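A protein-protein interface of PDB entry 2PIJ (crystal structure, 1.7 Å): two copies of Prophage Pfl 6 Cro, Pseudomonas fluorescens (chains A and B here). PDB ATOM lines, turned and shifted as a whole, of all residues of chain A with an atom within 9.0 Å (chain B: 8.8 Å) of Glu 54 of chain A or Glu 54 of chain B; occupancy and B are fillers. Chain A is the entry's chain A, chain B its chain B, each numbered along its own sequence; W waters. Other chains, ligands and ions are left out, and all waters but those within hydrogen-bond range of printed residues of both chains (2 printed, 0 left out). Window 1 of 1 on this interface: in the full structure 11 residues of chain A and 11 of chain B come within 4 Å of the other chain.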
ATOM      1  N   LEU A   6     -16.101  24.204  14.759  1.00  0.00           N
ATOM      2  CA  LEU A   6     -14.674  24.077  14.328  1.00  0.00           C
ATOM      3  C   LEU A   6     -14.571  23.766  12.798  1.00  0.00           C
ATOM      4  O   LEU A   6     -13.662  24.312  12.131  1.00  0.00           O
ATOM      5  CB  LEU A   6     -14.002  22.953  15.136  1.00  0.00           C
ATOM      6  CG  LEU A   6     -12.579  22.549  14.703  1.00  0.00           C
ATOM      7  CD1 LEU A   6     -11.647  23.811  14.613  1.00  0.00           C
ATOM      8  CD2 LEU A   6     -12.027  21.436  15.672  1.00  0.00           C
ATOM      9  N   GLN A  32      -6.174  16.354  16.782  1.00  0.00           N
ATOM     10  CA  GLN A  32      -6.876  15.342  17.558  1.00  0.00           C
ATOM     11  C   GLN A  32      -8.401  15.605  17.641  1.00  0.00           C
ATOM     12  O   GLN A  32      -9.194  14.657  17.491  1.00  0.00           O
ATOM     13  CB  GLN A  32      -6.163  15.194  18.918  1.00  0.00           C
ATOM     14  CG  GLN A  32      -6.653  14.083  19.775  1.00  0.00           C
ATOM     15  CD  GLN A  32      -8.089  14.316  20.187  1.00  0.00           C
ATOM     16  OE1 GLN A  32      -8.479  15.456  20.438  1.00  0.00           O
ATOM     17  NE2 GLN A  32      -8.903  13.258  20.188  1.00  0.00           N
ATOM     18  N   MET A  33      -8.806  16.872  17.838  1.00  0.00           N
ATOM     19  CA  MET A  33     -10.209  17.234  17.908  1.00  0.00           C
ATOM     20  C   MET A  33     -10.929  16.975  16.595  1.00  0.00           C
ATOM     21  O   MET A  33     -12.060  16.501  16.566  1.00  0.00           O
ATOM     22  CB  MET A  33     -10.315  18.710  18.254  1.00  0.00           C
ATOM     23  CG  MET A  33      -9.901  18.965  19.695  1.00  0.00           C
ATOM     24  SD  MET A  33      -9.650  20.851  20.085  1.00  0.00           S
ATOM     25  CE  MET A  33      -8.363  20.632  21.528  1.00  0.00           C
ATOM     26  N   ALA A  36     -11.376  13.126  16.137  1.00  0.00           N
ATOM     27  CA  ALA A  36     -12.225  12.392  17.099  1.00  0.00           C
ATOM     28  C   ALA A  36     -13.649  12.897  17.067  1.00  0.00           C
ATOM     29  O   ALA A  36     -14.494  12.464  17.878  1.00  0.00           O
ATOM     30  CB  ALA A  36     -11.673  12.508  18.507  1.00  0.00           C
ATOM     31  N   GLY A  37     -13.902  13.799  16.123  1.00  0.00           N
ATOM     32  CA  GLY A  37     -15.240  14.393  15.935  1.00  0.00           C
ATOM     33  C   GLY A  37     -15.696  15.256  17.104  1.00  0.00           C
ATOM     34  O   GLY A  37     -16.892  15.370  17.348  1.00  0.00           O
ATOM     35  N   ARG A  38     -14.759  15.840  17.851  1.00  0.00           N
ATOM     36  CA  ARG A  38     -15.157  16.481  19.090  1.00  0.00           C
ATOM     37  C   ARG A  38     -15.917  17.720  18.786  1.00  0.00           C
ATOM     38  O   ARG A  38     -15.751  18.315  17.714  1.00  0.00           O
ATOM     39  CB  ARG A  38     -13.976  16.724  20.040  1.00  0.00           C
ATOM     40  CG  ARG A  38     -13.309  15.367  20.415  1.00  0.00           C
ATOM     41  CD  ARG A  38     -11.911  15.566  20.953  1.00  0.00           C
ATOM     42  NE  ARG A  38     -11.922  16.403  22.148  1.00  0.00           N
ATOM     43  CZ  ARG A  38     -10.853  16.640  22.914  1.00  0.00           C
ATOM     44  NH1 ARG A  38      -9.669  16.075  22.662  1.00  0.00           N
ATOM     45  NH2 ARG A  38     -10.977  17.421  23.970  1.00  0.00           N
ATOM     46  N   SER A  39     -16.773  18.098  19.726  1.00  0.00           N
ATOM     47  CA  SER A  39     -17.730  19.178  19.495  1.00  0.00           C
ATOM     48  C   SER A  39     -17.090  20.464  19.961  1.00  0.00           C
ATOM     49  O   SER A  39     -17.139  20.799  21.148  1.00  0.00           O
ATOM     50  CB  SER A  39     -19.050  18.883  20.253  1.00  0.00           C
ATOM     51  OG  SER A  39     -19.675  17.663  19.816  1.00  0.00           O
ATOM     52  N   ILE A  40     -16.463  21.159  19.011  1.00  0.00           N
ATOM     53  CA  ILE A  40     -15.664  22.334  19.345  1.00  0.00           C
ATOM     54  C   ILE A  40     -16.296  23.553  18.682  1.00  0.00           C
ATOM     55  O   ILE A  40     -16.580  23.550  17.459  1.00  0.00           O
ATOM     56  CB  ILE A  40     -14.132  22.175  18.955  1.00  0.00           C
ATOM     57  CG1 ILE A  40     -13.409  20.887  19.495  1.00  0.00           C
ATOM     58  CG2 ILE A  40     -13.333  23.483  19.182  1.00  0.00           C
ATOM     59  CD1 ILE A  40     -13.476  20.633  21.006  1.00  0.00           C
ATOM     60  N   GLU A  41     -16.521  24.580  19.485  1.00  0.00           N
ATOM     61  CA  GLU A  41     -17.110  25.832  19.056  1.00  0.00           C
ATOM     62  C   GLU A  41     -16.040  26.950  19.167  1.00  0.00           C
ATOM     63  O   GLU A  41     -15.399  27.038  20.214  1.00  0.00           O
ATOM     64  CB  GLU A  41     -18.346  26.073  19.894  1.00  0.00           C
ATOM     65  CG  GLU A  41     -18.968  27.432  19.819  1.00  0.00           C
ATOM     66  CD  GLU A  41     -20.387  27.370  20.382  1.00  0.00           C
ATOM     67  OE1 GLU A  41     -20.574  27.188  21.605  1.00  0.00           O
ATOM     68  OE2 GLU A  41     -21.321  27.444  19.578  1.00  0.00           O
ATOM     69  N   ILE A  42     -15.845  27.750  18.094  1.00  0.00           N
ATOM     70  CA  ILE A  42     -14.862  28.860  18.070  1.00  0.00           C
ATOM     71  C   ILE A  42     -15.657  30.135  18.133  1.00  0.00           C
ATOM     72  O   ILE A  42     -16.629  30.291  17.366  1.00  0.00           O
ATOM     73  CB  ILE A  42     -14.005  28.862  16.763  1.00  0.00           C
ATOM     74  CG1 ILE A  42     -13.303  27.506  16.551  1.00  0.00           C
ATOM     75  CG2 ILE A  42     -12.996  30.019  16.775  1.00  0.00           C
ATOM     76  CD1 ILE A  42     -12.336  27.030  17.637  1.00  0.00           C
ATOM     77  N   GLU A  51     -11.630  32.533  20.814  1.00  0.00           N
ATOM     78  CA  GLU A  51     -11.538  31.584  21.902  1.00  0.00           C
ATOM     79  C   GLU A  51     -12.269  30.295  21.458  1.00  0.00           C
ATOM     80  O   GLU A  51     -13.021  30.287  20.451  1.00  0.00           O
ATOM     81  CB  GLU A  51     -12.060  32.174  23.247  1.00  0.00           C
ATOM     82  CG  GLU A  51     -13.473  31.816  23.528  1.00  0.00           C
ATOM     83  CD  GLU A  51     -14.015  32.416  24.822  1.00  0.00           C
ATOM     84  OE1 GLU A  51     -14.177  33.660  24.842  1.00  0.00           O
ATOM     85  OE2 GLU A  51     -14.288  31.645  25.781  1.00  0.00           O
ATOM     86  N   ALA A  52     -11.888  29.190  22.085  1.00  0.00           N
ATOM     87  CA  ALA A  52     -12.453  27.878  21.767  1.00  0.00           C
ATOM     88  C   ALA A  52     -13.080  27.292  23.030  1.00  0.00           C
ATOM     89  O   ALA A  52     -12.544  27.476  24.143  1.00  0.00           O
ATOM     90  CB  ALA A  52     -11.393  26.924  21.235  1.00  0.00           C
ATOM     91  N   ASN A  53     -14.203  26.600  22.839  1.00  0.00           N
ATOM     92  CA  ASN A  53     -14.834  25.723  23.867  1.00  0.00           C
ATOM     93  C   ASN A  53     -15.285  24.388  23.297  1.00  0.00           C
ATOM     94  O   ASN A  53     -15.681  24.268  22.128  1.00  0.00           O
ATOM     95  CB  ASN A  53     -16.033  26.401  24.585  1.00  0.00           C
ATOM     96  CG  ASN A  53     -15.627  27.673  25.317  1.00  0.00           C
ATOM     97  OD1 ASN A  53     -15.197  27.639  26.459  1.00  0.00           O
ATOM     98  ND2 ASN A  53     -15.772  28.805  24.650  1.00  0.00           N
ATOM     99  N   GLU A  54     -15.188  23.361  24.128  1.00  0.00           N
ATOM    100  CA  GLU A  54     -15.789  22.066  23.814  1.00  0.00           C
ATOM    101  C   GLU A  54     -17.127  21.986  24.515  1.00  0.00           C
ATOM    102  O   GLU A  54     -17.271  22.156  25.742  1.00  0.00           O
ATOM    103  CB  GLU A  54     -14.873  20.905  24.253  1.00  0.00           C
ATOM    104  CG  GLU A  54     -15.441  19.530  23.922  1.00  0.00           C
ATOM    105  CD  GLU A  54     -14.466  18.400  24.214  1.00  0.00           C
ATOM    106  OE1 GLU A  54     -13.612  18.557  25.105  1.00  0.00           O
ATOM    107  OE2 GLU A  54     -14.561  17.351  23.529  1.00  0.00           O
ATOM    108  N   ILE A  55     -18.100  21.599  23.729  1.00  0.00           N
ATOM    109  CA  ILE A  55     -19.456  21.273  24.200  1.00  0.00           C
ATOM    110  C   ILE A  55     -19.555  19.741  24.479  1.00  0.00           C
ATOM    111  O   ILE A  55     -19.598  18.898  23.550  1.00  0.00           O
ATOM    112  CB  ILE A  55     -20.519  21.705  23.160  1.00  0.00           C
ATOM    113  CG1 ILE A  55     -20.307  23.181  22.746  1.00  0.00           C
ATOM    114  CG2 ILE A  55     -21.928  21.499  23.739  1.00  0.00           C
ATOM    115  CD1 ILE A  55     -21.183  23.606  21.501  1.00  0.00           C
ATOM    116  N   ARG A  56     -19.630  19.391  25.770  1.00  0.00           N
ATOM    117  CA  ARG A  56     -19.719  18.009  26.225  1.00  0.00           C
ATOM    118  C   ARG A  56     -21.130  17.692  26.704  1.00  0.00           C
ATOM    119  O   ARG A  56     -21.550  18.258  27.713  1.00  0.00           O
ATOM    120  CB  ARG A  56     -18.663  17.652  27.276  1.00  0.00           C
ATOM    121  CG  ARG A  56     -17.250  18.076  26.911  1.00  0.00           C
ATOM    122  CD  ARG A  56     -16.236  17.254  27.682  1.00  0.00           C
ATOM    123  NE  ARG A  56     -16.921  16.648  28.822  1.00  0.00           N
ATOM    124  CZ  ARG A  56     -16.649  15.447  29.315  1.00  0.00           C
ATOM    125  NH1 ARG A  56     -15.655  14.716  28.804  1.00  0.00           N
ATOM    126  NH2 ARG A  56     -17.364  14.989  30.336  1.00  0.00           N
ATOM    127  N   PRO A  57     -21.872  16.837  25.955  1.00  0.00           N
ATOM    128  CA  PRO A  57     -23.204  16.445  26.346  1.00  0.00           C
ATOM    129  C   PRO A  57     -23.210  15.757  27.742  1.00  0.00           C
ATOM    130  O   PRO A  57     -22.318  14.955  28.056  1.00  0.00           O
ATOM    131  CB  PRO A  57     -23.612  15.429  25.271  1.00  0.00           C
ATOM    132  CG  PRO A  57     -22.340  14.992  24.646  1.00  0.00           C
ATOM    133  CD  PRO A  57     -21.470  16.199  24.697  1.00  0.00           C
ATOM    134  N   ILE A  58     -24.258  16.016  28.511  1.00  0.00           N
ATOM    135  CA  ILE A  58     -24.508  15.432  29.815  1.00  0.00           C
ATOM    136  C   ILE A  58     -25.918  14.770  29.758  1.00  0.00           C
ATOM    137  O   ILE A  58     -26.938  15.460  29.492  1.00  0.00           O
ATOM    138  CB  ILE A  58     -24.505  16.512  30.943  1.00  0.00           C
ATOM    139  CG1 ILE A  58     -23.204  17.332  30.996  1.00  0.00           C
ATOM    140  CG2 ILE A  58     -24.933  15.940  32.294  1.00  0.00           C
ATOM    141  CD1 ILE A  58     -21.930  16.547  31.362  1.00  0.00           C
ATOM    142  N   PRO A  59     -25.998  13.454  30.036  1.00  0.00           N
ATOM    143  CA  PRO A  59     -24.963  12.485  30.490  1.00  0.00           C
ATOM    144  C   PRO A  59     -23.850  12.263  29.464  1.00  0.00           C
ATOM    145  O   PRO A  59     -24.226  11.961  28.279  1.00  0.00           O
ATOM    146  CB  PRO A  59     -25.761  11.188  30.699  1.00  0.00           C
ATOM    147  CG  PRO A  59     -26.959  11.318  29.831  1.00  0.00           C
ATOM    148  CD  PRO A  59     -27.309  12.784  29.855  1.00  0.00           C
ATOM    149  N   GLN B  32     -22.923  16.208  42.136  1.00  0.00           N
ATOM    150  CA  GLN B  32     -21.501  16.329  41.817  1.00  0.00           C
ATOM    151  C   GLN B  32     -21.166  17.576  40.951  1.00  0.00           C
ATOM    152  O   GLN B  32     -20.137  18.231  41.171  1.00  0.00           O
ATOM    153  CB  GLN B  32     -20.976  15.035  41.186  1.00  0.00           C
ATOM    154  CG  GLN B  32     -19.447  14.942  41.081  1.00  0.00           C
ATOM    155  CD  GLN B  32     -18.860  15.860  39.978  1.00  0.00           C
ATOM    156  OE1 GLN B  32     -19.520  16.112  38.963  1.00  0.00           O
ATOM    157  NE2 GLN B  32     -17.622  16.352  40.179  1.00  0.00           N
ATOM    158  N   MET B  33     -22.015  17.893  39.968  1.00  0.00           N
ATOM    159  CA  MET B  33     -21.778  19.052  39.085  1.00  0.00           C
ATOM    160  C   MET B  33     -21.877  20.372  39.856  1.00  0.00           C
ATOM    161  O   MET B  33     -21.017  21.242  39.717  1.00  0.00           O
ATOM    162  CB  MET B  33     -22.724  19.030  37.902  1.00  0.00           C
ATOM    163  CG  MET B  33     -22.480  17.840  37.009  1.00  0.00           C
ATOM    164  SD  MET B  33     -24.007  17.566  35.831  1.00  0.00           S
ATOM    165  CE  MET B  33     -25.378  18.311  37.031  1.00  0.00           C
ATOM    166  N   ALA B  36     -18.563  20.662  42.362  1.00  0.00           N
ATOM    167  CA  ALA B  36     -17.323  20.962  41.648  1.00  0.00           C
ATOM    168  C   ALA B  36     -17.365  22.234  40.789  1.00  0.00           C
ATOM    169  O   ALA B  36     -16.407  22.509  40.077  1.00  0.00           O
ATOM    170  CB  ALA B  36     -16.907  19.761  40.796  1.00  0.00           C
ATOM    171  N   GLY B  37     -18.469  22.990  40.835  1.00  0.00           N
ATOM    172  CA  GLY B  37     -18.616  24.218  40.029  1.00  0.00           C
ATOM    173  C   GLY B  37     -18.340  23.999  38.545  1.00  0.00           C
ATOM    174  O   GLY B  37     -17.661  24.805  37.883  1.00  0.00           O
ATOM    175  N   ARG B  38     -18.830  22.883  38.018  1.00  0.00           N
ATOM    176  CA  ARG B  38     -18.642  22.600  36.626  1.00  0.00           C
ATOM    177  C   ARG B  38     -19.469  23.557  35.764  1.00  0.00           C
ATOM    178  O   ARG B  38     -20.555  23.998  36.179  1.00  0.00           O
ATOM    179  CB  ARG B  38     -18.947  21.127  36.340  1.00  0.00           C
ATOM    180  CG  ARG B  38     -17.881  20.192  36.965  1.00  0.00           C
ATOM    181  CD  ARG B  38     -18.366  18.716  36.986  1.00  0.00           C
ATOM    182  NE  ARG B  38     -18.665  18.209  35.644  1.00  0.00           N
ATOM    183  CZ  ARG B  38     -19.072  16.974  35.368  1.00  0.00           C
ATOM    184  NH1 ARG B  38     -19.205  16.060  36.338  1.00  0.00           N
ATOM    185  NH2 ARG B  38     -19.306  16.627  34.102  1.00  0.00           N
ATOM    186  N   SER B  39     -18.967  23.916  34.581  1.00  0.00           N
ATOM    187  CA  SER B  39     -19.716  24.866  33.739  1.00  0.00           C
ATOM    188  C   SER B  39     -20.839  24.168  32.964  1.00  0.00           C
ATOM    189  O   SER B  39     -20.713  23.882  31.776  1.00  0.00           O
ATOM    190  CB  SER B  39     -18.826  25.736  32.808  1.00  0.00           C
ATOM    191  OG  SER B  39     -18.397  26.950  33.482  1.00  0.00           O
ATOM    192  N   ILE B  40     -21.960  23.928  33.636  1.00  0.00           N
ATOM    193  CA  ILE B  40     -23.057  23.203  33.015  1.00  0.00           C
ATOM    194  C   ILE B  40     -24.164  24.175  32.603  1.00  0.00           C
ATOM    195  O   ILE B  40     -24.604  25.029  33.402  1.00  0.00           O
ATOM    196  CB  ILE B  40     -23.606  22.081  33.998  1.00  0.00           C
ATOM    197  CG1 ILE B  40     -22.507  21.111  34.570  1.00  0.00           C
ATOM    198  CG2 ILE B  40     -24.808  21.371  33.356  1.00  0.00           C
ATOM    199  CD1 ILE B  40     -21.885  20.117  33.620  1.00  0.00           C
ATOM    200  N   GLU B  41     -24.614  24.045  31.339  1.00  0.00           N
ATOM    201  CA  GLU B  41     -25.643  24.864  30.755  1.00  0.00           C
ATOM    202  C   GLU B  41     -26.868  23.989  30.497  1.00  0.00           C
ATOM    203  O   GLU B  41     -26.792  22.872  29.958  1.00  0.00           O
ATOM    204  CB  GLU B  41     -25.130  25.521  29.471  1.00  0.00           C
ATOM    205  CG  GLU B  41     -26.183  26.407  28.749  1.00  0.00           C
ATOM    206  CD  GLU B  41     -25.831  26.643  27.317  1.00  0.00           C
ATOM    207  OE1 GLU B  41     -25.969  25.706  26.482  1.00  0.00           O
ATOM    208  OE2 GLU B  41     -25.457  27.777  26.996  1.00  0.00           O
ATOM    209  N   ILE B  42     -28.006  24.468  30.953  1.00  0.00           N
ATOM    210  CA  ILE B  42     -29.236  23.765  30.737  1.00  0.00           C
ATOM    211  C   ILE B  42     -30.037  24.428  29.570  1.00  0.00           C
ATOM    212  O   ILE B  42     -30.278  25.622  29.549  1.00  0.00           O
ATOM    213  CB  ILE B  42     -30.099  23.731  32.047  1.00  0.00           C
ATOM    214  CG1 ILE B  42     -29.329  23.056  33.208  1.00  0.00           C
ATOM    215  CG2 ILE B  42     -31.457  23.067  31.754  1.00  0.00           C
ATOM    216  CD1 ILE B  42     -28.992  21.577  33.021  1.00  0.00           C
ATOM    217  N   GLU B  51     -32.097  19.572  27.783  1.00  0.00           N
ATOM    218  CA  GLU B  51     -30.755  19.067  27.546  1.00  0.00           C
ATOM    219  C   GLU B  51     -29.735  19.730  28.464  1.00  0.00           C
ATOM    220  O   GLU B  51     -29.971  20.814  29.008  1.00  0.00           O
ATOM    221  CB  GLU B  51     -30.299  19.229  26.097  1.00  0.00           C
ATOM    222  CG  GLU B  51     -31.166  18.497  25.097  1.00  0.00           C
ATOM    223  CD  GLU B  51     -30.646  18.593  23.698  1.00  0.00           C
ATOM    224  OE1 GLU B  51     -30.239  19.687  23.281  1.00  0.00           O
ATOM    225  OE2 GLU B  51     -30.747  17.574  22.992  1.00  0.00           O
ATOM    226  N   ALA B  52     -28.604  19.089  28.605  1.00  0.00           N
ATOM    227  CA  ALA B  52     -27.533  19.622  29.484  1.00  0.00           C
ATOM    228  C   ALA B  52     -26.203  19.418  28.723  1.00  0.00           C
ATOM    229  O   ALA B  52     -25.988  18.363  28.106  1.00  0.00           O
ATOM    230  CB  ALA B  52     -27.517  18.981  30.899  1.00  0.00           C
ATOM    231  N   ASN B  53     -25.296  20.369  28.918  1.00  0.00           N
ATOM    232  CA  ASN B  53     -23.968  20.402  28.263  1.00  0.00           C
ATOM    233  C   ASN B  53     -23.003  21.076  29.203  1.00  0.00           C
ATOM    234  O   ASN B  53     -23.314  22.096  29.832  1.00  0.00           O
ATOM    235  CB  ASN B  53     -24.032  21.236  26.941  1.00  0.00           C
ATOM    236  CG  ASN B  53     -24.821  20.547  25.856  1.00  0.00           C
ATOM    237  OD1 ASN B  53     -24.349  19.563  25.276  1.00  0.00           O
ATOM    238  ND2 ASN B  53     -25.977  21.119  25.507  1.00  0.00           N
ATOM    239  N   GLU B  54     -21.816  20.541  29.287  1.00  0.00           N
ATOM    240  CA  GLU B  54     -20.718  21.192  29.946  1.00  0.00           C
ATOM    241  C   GLU B  54     -19.986  21.996  28.862  1.00  0.00           C
ATOM    242  O   GLU B  54     -19.685  21.429  27.761  1.00  0.00           O
ATOM    243  CB  GLU B  54     -19.795  20.125  30.513  1.00  0.00           C
ATOM    244  CG  GLU B  54     -18.619  20.655  31.345  1.00  0.00           C
ATOM    245  CD  GLU B  54     -17.965  19.549  32.175  1.00  0.00           C
ATOM    246  OE1 GLU B  54     -17.829  18.404  31.685  1.00  0.00           O
ATOM    247  OE2 GLU B  54     -17.583  19.822  33.337  1.00  0.00           O
ATOM    248  N   ILE B  55     -19.746  23.269  29.131  1.00  0.00           N
ATOM    249  CA  ILE B  55     -18.901  24.122  28.278  1.00  0.00           C
ATOM    250  C   ILE B  55     -17.483  24.198  28.853  1.00  0.00           C
ATOM    251  O   ILE B  55     -17.239  24.769  29.929  1.00  0.00           O
ATOM    252  CB  ILE B  55     -19.446  25.593  28.123  1.00  0.00           C
ATOM    253  CG1 ILE B  55     -20.940  25.712  27.857  1.00  0.00           C
ATOM    254  CG2 ILE B  55     -18.732  26.339  27.043  1.00  0.00           C
ATOM    255  CD1 ILE B  55     -21.695  24.626  26.912  1.00  0.00           C
ATOM    256  N   ARG B  56     -16.558  23.596  28.123  1.00  0.00           N
ATOM    257  CA  ARG B  56     -15.175  23.504  28.569  1.00  0.00           C
ATOM    258  C   ARG B  56     -14.231  24.344  27.725  1.00  0.00           C
ATOM    259  O   ARG B  56     -14.124  24.122  26.533  1.00  0.00           O
ATOM    260  CB  ARG B  56     -14.741  22.031  28.513  1.00  0.00           C
ATOM    261  CG  ARG B  56     -15.621  21.095  29.370  1.00  0.00           C
ATOM    262  CD  ARG B  56     -14.743  20.243  30.287  1.00  0.00           C
ATOM    263  NE  ARG B  56     -13.712  19.550  29.520  1.00  0.00           N
ATOM    264  CZ  ARG B  56     -13.505  18.237  29.553  1.00  0.00           C
ATOM    265  NH1 ARG B  56     -14.245  17.441  30.326  1.00  0.00           N
ATOM    266  NH2 ARG B  56     -12.527  17.719  28.817  1.00  0.00           N
ATOM    267  N   PRO B  57     -13.511  25.314  28.346  1.00  0.00           N
ATOM    268  CA  PRO B  57     -12.578  26.100  27.520  1.00  0.00           C
ATOM    269  C   PRO B  57     -11.404  25.264  26.995  1.00  0.00           C
ATOM    270  O   PRO B  57     -11.016  24.258  27.609  1.00  0.00           O
ATOM    271  CB  PRO B  57     -12.094  27.192  28.480  1.00  0.00           C
ATOM    272  CG  PRO B  57     -12.407  26.718  29.794  1.00  0.00           C
ATOM    273  CD  PRO B  57     -13.495  25.746  29.748  1.00  0.00           C
ATOM    274  N   ILE B  58     -10.883  25.702  25.850  1.00  0.00           N
ATOM    275  CA  ILE B  58      -9.758  25.098  25.177  1.00  0.00           C
ATOM    276  C   ILE B  58      -8.774  26.249  24.875  1.00  0.00           C
ATOM    277  O   ILE B  58      -9.076  27.166  24.093  1.00  0.00           O
ATOM    278  CB  ILE B  58     -10.131  24.347  23.826  1.00  0.00           C
ATOM    279  CG1 ILE B  58     -11.252  23.287  24.020  1.00  0.00           C
ATOM    280  CG2 ILE B  58      -8.820  23.851  23.062  1.00  0.00           C
ATOM    281  CD1 ILE B  58     -10.852  22.015  24.791  1.00  0.00           C
ATOM    282  N   PRO B  59      -7.610  26.216  25.518  1.00  0.00           N
ATOM    283  CA  PRO B  59      -7.209  25.188  26.472  1.00  0.00           C
ATOM    284  C   PRO B  59      -7.898  25.324  27.829  1.00  0.00           C
ATOM    285  O   PRO B  59      -8.545  26.359  28.118  1.00  0.00           O
ATOM    286  CB  PRO B  59      -5.699  25.418  26.621  1.00  0.00           C
ATOM    287  CG  PRO B  59      -5.518  26.838  26.347  1.00  0.00           C
ATOM    288  CD  PRO B  59      -6.576  27.252  25.367  1.00  0.00           C
ATOM    289  N   ALA B  60      -7.803  24.274  28.633  1.00  0.00           N
ATOM    290  CA  ALA B  60      -8.355  24.300  30.000  1.00  0.00           C
ATOM    291  C   ALA B  60      -7.454  25.081  30.944  1.00  0.00           C
ATOM    292  O   ALA B  60      -6.534  25.773  30.460  1.00  0.00           O
ATOM    293  CB  ALA B  60      -8.574  22.881  30.541  1.00  0.00           C
HETATM  294  O   HOH W   1      -9.919  29.528  24.172  1.00  0.00           O
HETATM  295  O   HOH W   2     -28.719  16.170  27.834  1.00  0.00           O
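Among the printed residues, pairs that only touch across the chains: Asn 53 of chain A with Arg 56 of chain B (3.2 Å), Arg 56 of chain A with Asn 53 of chain B (3.3 Å), Ile 55 of chain A with Asn 53 of chain B (3.5 Å), Pro 57 of chain A with Asn 53 of chain B (3.5 Å), Ile 55 of chain A with Glu 54 of chain B (3.6 Å), Met 33 of chain A with Ile 58 of chain B (3.6 Å), Glu 54 of chain A with Ile 55 of chain B (3.6 Å), Ala 52 of chain A with Pro 57 of chain B (3.6 Å), Asn 53 of chain A with Ile 55 of chain B (3.7 Å), Ile 58 of chain A with Arg 38 of chain B (3.8 Å), Pro 57 of chain A with Ala 52 of chain B (3.8 Å), Ile 58 of chain A with Glu 54 of chain B (3.9 Å) and Glu 54 of chain A with Ile 58 of chain B (3.9 Å).
The backbone NH (N) of Arg 38 of chain A is in hydrogen-bond range of the backbone carbonyl oxygen (O) of Met 33 of chain A, at 3.1 Å.
The backbone NH of Ile 55 of chain A lies within hydrogen-bond range of the backbone carbonyl oxygen of Ser 39 of chain A, at 2.9 Å.
O of Asn 53 of chain A is in hydrogen-bond range of N of Glu 41 of chain A, at 2.8 Å.
The backbone carbonyl oxygen of Ser 39 of chain B is in hydrogen-bond range of the backbone NH of Ile 55 of chain B (2.9 Å).
OE1 of Glu 54 of chain B is in salt-bridge range of NH1 of Arg 56 of chain B, 3.95 Å away.
Met 33 of chain A touches Ile 58 of chain B, but with the chains exchanged Ile 58 of chain A does not touch Met 33 of chain B (4.001 Å).
Glu 54 of chain A touches its own counterpart, Glu 54 of chain B.
Glu 54 of chain A touches Ile 55 of chain B, and with the chains exchanged Ile 55 of chain A touches Glu 54 of chain B.
Glu 54 of chain A touches Ile 58 of chain B, and with the chains exchanged Ile 58 of chain A touches Glu 54 of chain B.
Water W1 bridges O of Ile 58 of chain B (2.5 Å) and N of Ala 52 of chain A (2.9 Å).
Water W2 lies within hydrogen-bond range of O of Ile 58 of chain A (2.5 Å) and N of Ala 52 of chain B (3.0 Å).
Of chain B, only Glu 54, Ile 55, Arg 56 and Ile 58 come within 4 Å of Glu 54 of chain A.
Glu 54 of chain B touches just these residues of chain A: Glu 54, Ile 55, Arg 56 and Ile 58.
Of the printed residues of chain A, Arg 56 of chain B touches Asn 53, Glu 54 and Arg 56.
Of the printed residues of chain A, Ile 58 of chain B touches Met 33 (3.6 Å), Ala 52 (3.0 Å) and Glu 54 (3.9 Å).
Of the printed residues of chain B, Ile 58 of chain A touches Arg 38, Ala 52 and Glu 54.
Of the printed residues of chain A, Ala 52 of chain B touches Pro 57 (3.8 Å) and Ile 58 (2.9 Å).
Printed residues of chain B within 4 Å of Asn 53 of chain A: Ile 55 (3.7 Å), Arg 56 (3.2 Å) and Pro 57 (3.2 Å).
The nearest residue of chain A that does not touch Glu 54 of chain B is Pro 57 of chain A (5.0 Å).
Hydrophobic or aromatic side chains of chain A that line the printed part of chain B: Met 33, Ala 52, Ile 55 and Ile 58.
Along chain A the printed residues that touch a printed residue of chain B span positions 33 to 58.
Hydrophobic or aromatic side chains of chain B that line the printed part of chain A: Ala 52, Ile 55, Pro 57 and Ile 58.
Among the printed residues, 20 pairs touch across the chains.
Among the printed residues, Asp or Glu carboxylates within 4 Å of a Lys or Arg side-chain nitrogen of the other chain: Glu 54 of chain A with Arg 56 of chain B (3.96 Å) and Arg 56 of chain A with Glu 54 of chain B (3.5 Å).
O of Ala 52 of chain A is in hydrogen-bond range of N of Ile 58 of chain B (3.0 Å).
NH2 of Arg 56 of chain B is in salt-bridge range of OE1 of Glu 54 of chain A, at 3.96 Å.
The guanidinium group of Arg 56 of chain A is in salt-bridge range of the side-chain carboxylate of Glu 54 of chain B (3.5 Å).
The backbone NH (N) of Ile 58 of chain A sits at hydrogen-bond distance from the backbone carbonyl oxygen (O) of Ala 52 of chain B (2.9 Å).
N of Pro 57 of chain B lies close to OD1 of Asn 53 of chain A (3.4 Å).
O of Glu 54 of chain A lies close to O of Glu 54 of chain B (3.2 Å).
NH1 of Arg 56 of chain B lies close to NE of Arg 56 of chain A, 3.2 Å away.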
